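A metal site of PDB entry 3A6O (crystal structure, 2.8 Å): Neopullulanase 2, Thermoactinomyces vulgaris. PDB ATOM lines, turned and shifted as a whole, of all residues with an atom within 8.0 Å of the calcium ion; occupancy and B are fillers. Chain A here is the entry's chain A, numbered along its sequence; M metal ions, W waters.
The calcium ion is bound by O of Gly 169 (2.3 Å), OD2 of Asp 171 (2.3 Å), OD2 of Asp 149 (2.3 Å), water W1 (2.5 Å), OD1 of Asn 143 (2.5 Å), OD1 of Asn 148 (2.5 Å) and O of Asp 145 (2.5 Å).
OD1 of Asp 171 sits at hydrogen-bond distance from N of Gly 174 (3.0 Å).
The side-chain carboxylate (OE1) of Glu 139 is in hydrogen-bond range of the backbone NH (N) of Gly 169.
OD1 of Asp 171 is in hydrogen-bond range of N of Lys 173 (3.3 Å).
OG of Ser 147 lies within hydrogen-bond range of OD1 of Asp 145 (2.7 Å).
N of Gly 144 is in hydrogen-bond range of OD1 of Asp 171 (3.0 Å).
The backbone NH of Asp 171 is in hydrogen-bond range of the backbone carbonyl oxygen of Ala 142, 2.8 Å away.
Water W1 bridges O of Gln 215 (2.4 Å) and O of Asn 148 (3.4 Å).
Of the 24 residues printed, 6 come within 4 Å of the calcium ion.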
ATOM      1  N   PRO A 138     -26.360 -20.296  24.552  1.00  0.00           N
ATOM      2  CA  PRO A 138     -25.010 -20.169  24.013  1.00  0.00           C
ATOM      3  C   PRO A 138     -24.505 -18.727  23.935  1.00  0.00           C
ATOM      4  O   PRO A 138     -23.393 -18.437  24.410  1.00  0.00           O
ATOM      5  CB  PRO A 138     -25.136 -20.689  22.624  1.00  0.00           C
ATOM      6  CG  PRO A 138     -26.307 -21.611  22.696  1.00  0.00           C
ATOM      7  CD  PRO A 138     -27.238 -21.025  23.649  1.00  0.00           C
ATOM      8  N   GLU A 139     -25.307 -17.799  23.392  1.00  0.00           N
ATOM      9  CA  GLU A 139     -24.856 -16.400  23.293  1.00  0.00           C
ATOM     10  C   GLU A 139     -24.244 -15.846  24.575  1.00  0.00           C
ATOM     11  O   GLU A 139     -23.385 -14.907  24.484  1.00  0.00           O
ATOM     12  CB  GLU A 139     -25.926 -15.463  22.779  1.00  0.00           C
ATOM     13  CG  GLU A 139     -25.419 -14.468  21.726  1.00  0.00           C
ATOM     14  CD  GLU A 139     -24.503 -13.302  22.259  1.00  0.00           C
ATOM     15  OE1 GLU A 139     -23.371 -13.100  21.742  1.00  0.00           O
ATOM     16  OE2 GLU A 139     -24.944 -12.563  23.153  1.00  0.00           O
ATOM     17  N   ALA A 142     -20.011 -18.788  27.230  1.00  0.00           N
ATOM     18  CA  ALA A 142     -18.541 -18.710  27.107  1.00  0.00           C
ATOM     19  C   ALA A 142     -18.169 -18.199  25.700  1.00  0.00           C
ATOM     20  O   ALA A 142     -18.510 -18.835  24.670  1.00  0.00           O
ATOM     21  CB  ALA A 142     -17.925 -20.075  27.347  1.00  0.00           C
ATOM     22  N   ASN A 143     -17.487 -17.063  25.657  1.00  0.00           N
ATOM     23  CA  ASN A 143     -16.782 -16.601  24.425  1.00  0.00           C
ATOM     24  C   ASN A 143     -15.451 -17.261  24.149  1.00  0.00           C
ATOM     25  O   ASN A 143     -14.468 -16.742  24.610  1.00  0.00           O
ATOM     26  CB  ASN A 143     -16.542 -15.072  24.472  1.00  0.00           C
ATOM     27  CG  ASN A 143     -16.334 -14.482  23.065  1.00  0.00           C
ATOM     28  OD1 ASN A 143     -15.965 -15.208  22.102  1.00  0.00           O
ATOM     29  ND2 ASN A 143     -16.613 -13.179  22.926  1.00  0.00           N
ATOM     30  N   GLY A 144     -15.373 -18.350  23.407  1.00  0.00           N
ATOM     31  CA  GLY A 144     -14.083 -19.013  23.227  1.00  0.00           C
ATOM     32  C   GLY A 144     -13.481 -18.581  21.898  1.00  0.00           C
ATOM     33  O   GLY A 144     -12.333 -18.843  21.561  1.00  0.00           O
ATOM     34  N   ASP A 145     -14.311 -17.973  21.057  1.00  0.00           N
ATOM     35  CA  ASP A 145     -13.798 -17.476  19.815  1.00  0.00           C
ATOM     36  C   ASP A 145     -14.247 -16.043  19.648  1.00  0.00           C
ATOM     37  O   ASP A 145     -15.352 -15.810  19.246  1.00  0.00           O
ATOM     38  CB  ASP A 145     -14.251 -18.332  18.669  1.00  0.00           C
ATOM     39  CG  ASP A 145     -13.638 -17.900  17.349  1.00  0.00           C
ATOM     40  OD1 ASP A 145     -12.982 -16.819  17.270  1.00  0.00           O
ATOM     41  OD2 ASP A 145     -13.806 -18.637  16.364  1.00  0.00           O
ATOM     42  N   PRO A 146     -13.383 -15.102  20.024  1.00  0.00           N
ATOM     43  CA  PRO A 146     -13.504 -13.659  19.878  1.00  0.00           C
ATOM     44  C   PRO A 146     -13.617 -13.213  18.410  1.00  0.00           C
ATOM     45  O   PRO A 146     -14.269 -12.126  18.164  1.00  0.00           O
ATOM     46  CB  PRO A 146     -12.161 -13.115  20.411  1.00  0.00           C
ATOM     47  CG  PRO A 146     -11.603 -14.298  21.193  1.00  0.00           C
ATOM     48  CD  PRO A 146     -12.141 -15.521  20.666  1.00  0.00           C
ATOM     49  N   SER A 147     -12.976 -13.958  17.471  1.00  0.00           N
ATOM     50  CA  SER A 147     -13.039 -13.554  16.055  1.00  0.00           C
ATOM     51  C   SER A 147     -14.406 -13.664  15.398  1.00  0.00           C
ATOM     52  O   SER A 147     -14.629 -13.029  14.367  1.00  0.00           O
ATOM     53  CB  SER A 147     -11.973 -14.187  15.195  1.00  0.00           C
ATOM     54  OG  SER A 147     -12.189 -15.549  15.035  1.00  0.00           O
ATOM     55  N   ASN A 148     -15.343 -14.435  15.988  1.00  0.00           N
ATOM     56  CA  ASN A 148     -16.657 -14.595  15.435  1.00  0.00           C
ATOM     57  C   ASN A 148     -17.705 -13.753  16.167  1.00  0.00           C
ATOM     58  O   ASN A 148     -18.907 -13.939  15.960  1.00  0.00           O
ATOM     59  CB  ASN A 148     -16.998 -16.050  15.388  1.00  0.00           C
ATOM     60  CG  ASN A 148     -17.310 -16.651  16.800  1.00  0.00           C
ATOM     61  OD1 ASN A 148     -17.475 -15.926  17.813  1.00  0.00           O
ATOM     62  ND2 ASN A 148     -17.417 -18.015  16.844  1.00  0.00           N
ATOM     63  N   ASP A 149     -17.258 -12.804  17.004  1.00  0.00           N
ATOM     64  CA  ASP A 149     -18.139 -12.002  17.868  1.00  0.00           C
ATOM     65  C   ASP A 149     -18.958 -11.123  16.987  1.00  0.00           C
ATOM     66  O   ASP A 149     -18.444 -10.604  15.991  1.00  0.00           O
ATOM     67  CB  ASP A 149     -17.299 -11.125  18.760  1.00  0.00           C
ATOM     68  CG  ASP A 149     -16.711 -11.885  19.937  1.00  0.00           C
ATOM     69  OD1 ASP A 149     -16.201 -11.226  20.848  1.00  0.00           O
ATOM     70  OD2 ASP A 149     -16.764 -13.134  19.980  1.00  0.00           O
ATOM     71  N   PRO A 150     -20.254 -10.979  17.263  1.00  0.00           N
ATOM     72  CA  PRO A 150     -21.165 -10.072  16.528  1.00  0.00           C
ATOM     73  C   PRO A 150     -20.761  -8.663  16.790  1.00  0.00           C
ATOM     74  O   PRO A 150     -20.067  -8.445  17.785  1.00  0.00           O
ATOM     75  CB  PRO A 150     -22.525 -10.301  17.194  1.00  0.00           C
ATOM     76  CG  PRO A 150     -22.441 -11.537  17.732  1.00  0.00           C
ATOM     77  CD  PRO A 150     -21.023 -11.761  18.219  1.00  0.00           C
ATOM     78  N   THR A 153     -20.627  -6.095  20.241  1.00  0.00           N
ATOM     79  CA  THR A 153     -20.503  -6.971  21.410  1.00  0.00           C
ATOM     80  C   THR A 153     -20.115  -6.118  22.592  1.00  0.00           C
ATOM     81  O   THR A 153     -19.130  -5.479  22.496  1.00  0.00           O
ATOM     82  CB  THR A 153     -19.451  -8.079  21.104  1.00  0.00           C
ATOM     83  OG1 THR A 153     -19.969  -8.984  20.084  1.00  0.00           O
ATOM     84  CG2 THR A 153     -19.034  -8.855  22.347  1.00  0.00           C
ATOM     85  N   TRP A 156     -17.844  -8.533  28.606  1.00  0.00           N
ATOM     86  CA  TRP A 156     -18.187  -9.697  29.345  1.00  0.00           C
ATOM     87  C   TRP A 156     -17.713  -9.512  30.726  1.00  0.00           C
ATOM     88  O   TRP A 156     -16.649 -10.014  31.093  1.00  0.00           O
ATOM     89  CB  TRP A 156     -17.505 -10.931  28.746  1.00  0.00           C
ATOM     90  CG  TRP A 156     -18.064 -12.260  29.250  1.00  0.00           C
ATOM     91  CD1 TRP A 156     -18.002 -12.745  30.533  1.00  0.00           C
ATOM     92  CD2 TRP A 156     -18.786 -13.263  28.484  1.00  0.00           C
ATOM     93  NE1 TRP A 156     -18.642 -13.966  30.617  1.00  0.00           N
ATOM     94  CE2 TRP A 156     -19.142 -14.305  29.373  1.00  0.00           C
ATOM     95  CE3 TRP A 156     -19.166 -13.376  27.144  1.00  0.00           C
ATOM     96  CZ2 TRP A 156     -19.863 -15.459  28.947  1.00  0.00           C
ATOM     97  CZ3 TRP A 156     -19.859 -14.529  26.728  1.00  0.00           C
ATOM     98  CH2 TRP A 156     -20.181 -15.541  27.620  1.00  0.00           C
ATOM     99  N   TYR A 168     -22.949 -10.674  23.720  1.00  0.00           N
ATOM    100  CA  TYR A 168     -21.669 -10.776  24.501  1.00  0.00           C
ATOM    101  C   TYR A 168     -20.572 -11.642  23.922  1.00  0.00           C
ATOM    102  O   TYR A 168     -19.466 -11.659  24.466  1.00  0.00           O
ATOM    103  CB  TYR A 168     -21.855 -11.119  25.977  1.00  0.00           C
ATOM    104  CG  TYR A 168     -22.660 -10.063  26.686  1.00  0.00           C
ATOM    105  CD1 TYR A 168     -22.027  -9.207  27.564  1.00  0.00           C
ATOM    106  CD2 TYR A 168     -24.052  -9.923  26.472  1.00  0.00           C
ATOM    107  CE1 TYR A 168     -22.726  -8.230  28.212  1.00  0.00           C
ATOM    108  CE2 TYR A 168     -24.781  -8.969  27.146  1.00  0.00           C
ATOM    109  CZ  TYR A 168     -24.095  -8.089  27.991  1.00  0.00           C
ATOM    110  OH  TYR A 168     -24.683  -7.046  28.668  1.00  0.00           O
ATOM    111  N   GLY A 169     -20.884 -12.317  22.811  1.00  0.00           N
ATOM    112  CA  GLY A 169     -19.977 -13.215  22.130  1.00  0.00           C
ATOM    113  C   GLY A 169     -19.904 -14.687  22.505  1.00  0.00           C
ATOM    114  O   GLY A 169     -18.998 -15.363  22.002  1.00  0.00           O
ATOM    115  N   GLY A 170     -20.835 -15.224  23.332  1.00  0.00           N
ATOM    116  CA  GLY A 170     -20.753 -16.632  23.706  1.00  0.00           C
ATOM    117  C   GLY A 170     -20.812 -17.443  22.431  1.00  0.00           C
ATOM    118  O   GLY A 170     -21.501 -17.017  21.475  1.00  0.00           O
ATOM    119  N   ASP A 171     -20.091 -18.540  22.333  1.00  0.00           N
ATOM    120  CA  ASP A 171     -20.162 -19.360  21.151  1.00  0.00           C
ATOM    121  C   ASP A 171     -19.864 -20.818  21.529  1.00  0.00           C
ATOM    122  O   ASP A 171     -19.583 -21.145  22.752  1.00  0.00           O
ATOM    123  CB  ASP A 171     -19.156 -18.929  20.122  1.00  0.00           C
ATOM    124  CG  ASP A 171     -17.809 -18.656  20.721  1.00  0.00           C
ATOM    125  OD1 ASP A 171     -17.227 -19.546  21.436  1.00  0.00           O
ATOM    126  OD2 ASP A 171     -17.277 -17.519  20.480  1.00  0.00           O
ATOM    127  N   LEU A 172     -19.883 -21.689  20.476  1.00  0.00           N
ATOM    128  CA  LEU A 172     -19.649 -23.108  20.650  1.00  0.00           C
ATOM    129  C   LEU A 172     -18.248 -23.495  21.127  1.00  0.00           C
ATOM    130  O   LEU A 172     -18.079 -24.470  21.813  1.00  0.00           O
ATOM    131  CB  LEU A 172     -20.064 -23.883  19.398  1.00  0.00           C
ATOM    132  CG  LEU A 172     -21.519 -23.773  18.914  1.00  0.00           C
ATOM    133  CD1 LEU A 172     -21.772 -24.771  17.781  1.00  0.00           C
ATOM    134  CD2 LEU A 172     -22.581 -24.005  20.089  1.00  0.00           C
ATOM    135  N   LYS A 173     -17.221 -22.768  20.696  1.00  0.00           N
ATOM    136  CA  LYS A 173     -15.831 -23.052  21.029  1.00  0.00           C
ATOM    137  C   LYS A 173     -15.682 -22.869  22.586  1.00  0.00           C
ATOM    138  O   LYS A 173     -14.989 -23.675  23.240  1.00  0.00           O
ATOM    139  CB  LYS A 173     -14.934 -22.148  20.170  1.00  0.00           C
ATOM    140  CG  LYS A 173     -13.411 -22.423  20.314  1.00  0.00           C
ATOM    141  CD  LYS A 173     -12.989 -23.889  20.650  1.00  0.00           C
ATOM    142  CE  LYS A 173     -11.524 -23.977  21.156  1.00  0.00           C
ATOM    143  NZ  LYS A 173     -10.870 -23.105  20.125  1.00  0.00           N
ATOM    144  N   GLY A 174     -16.411 -21.884  23.146  1.00  0.00           N
ATOM    145  CA  GLY A 174     -16.527 -21.664  24.581  1.00  0.00           C
ATOM    146  C   GLY A 174     -17.193 -22.847  25.328  1.00  0.00           C
ATOM    147  O   GLY A 174     -16.768 -23.188  26.474  1.00  0.00           O
ATOM    148  N   PRO A 214     -23.145 -18.491  12.127  1.00  0.00           N
ATOM    149  CA  PRO A 214     -21.751 -18.117  11.934  1.00  0.00           C
ATOM    150  C   PRO A 214     -21.137 -17.536  13.258  1.00  0.00           C
ATOM    151  O   PRO A 214     -19.967 -17.742  13.546  1.00  0.00           O
ATOM    152  CB  PRO A 214     -21.861 -16.984  10.957  1.00  0.00           C
ATOM    153  CG  PRO A 214     -22.993 -17.217  10.225  1.00  0.00           C
ATOM    154  CD  PRO A 214     -23.986 -17.856  11.086  1.00  0.00           C
ATOM    155  N   GLN A 215     -21.895 -16.806  14.050  1.00  0.00           N
ATOM    156  CA  GLN A 215     -21.265 -16.284  15.254  1.00  0.00           C
ATOM    157  C   GLN A 215     -21.259 -17.321  16.436  1.00  0.00           C
ATOM    158  O   GLN A 215     -20.812 -17.015  17.532  1.00  0.00           O
ATOM    159  CB  GLN A 215     -21.884 -14.943  15.614  1.00  0.00           C
ATOM    160  CG  GLN A 215     -22.999 -15.101  16.584  1.00  0.00           C
ATOM    161  CD  GLN A 215     -24.209 -14.092  16.398  1.00  0.00           C
ATOM    162  OE1 GLN A 215     -25.278 -14.233  17.097  1.00  0.00           O
ATOM    163  NE2 GLN A 215     -24.018 -13.070  15.490  1.00  0.00           N
ATOM    164  N   PHE A 216     -21.795 -18.516  16.233  1.00  0.00           N
ATOM    165  CA  PHE A 216     -21.660 -19.667  17.100  1.00  0.00           C
ATOM    166  C   PHE A 216     -20.623 -20.698  16.542  1.00  0.00           C
ATOM    167  O   PHE A 216     -20.001 -21.424  17.259  1.00  0.00           O
ATOM    168  CB  PHE A 216     -22.995 -20.363  17.247  1.00  0.00           C
ATOM    169  CG  PHE A 216     -23.935 -19.669  18.108  1.00  0.00           C
ATOM    170  CD1 PHE A 216     -23.503 -18.672  18.974  1.00  0.00           C
ATOM    171  CD2 PHE A 216     -25.250 -19.993  18.111  1.00  0.00           C
ATOM    172  CE1 PHE A 216     -24.459 -17.944  19.864  1.00  0.00           C
ATOM    173  CE2 PHE A 216     -26.187 -19.314  19.013  1.00  0.00           C
ATOM    174  CZ  PHE A 216     -25.777 -18.317  19.861  1.00  0.00           C
ATOM    175  N   GLY A 217     -20.412 -20.777  15.256  1.00  0.00           N
ATOM    176  CA  GLY A 217     -19.336 -21.611  14.803  1.00  0.00           C
ATOM    177  C   GLY A 217     -19.808 -22.081  13.471  1.00  0.00           C
ATOM    178  O   GLY A 217     -20.550 -21.303  12.789  1.00  0.00           O
HETATM  179 CA    CA M   1     -17.609 -15.295  20.233  1.00  0.00          CA
HETATM  180  O   HOH W   1     -19.688 -15.362  18.915  1.00  0.00           O
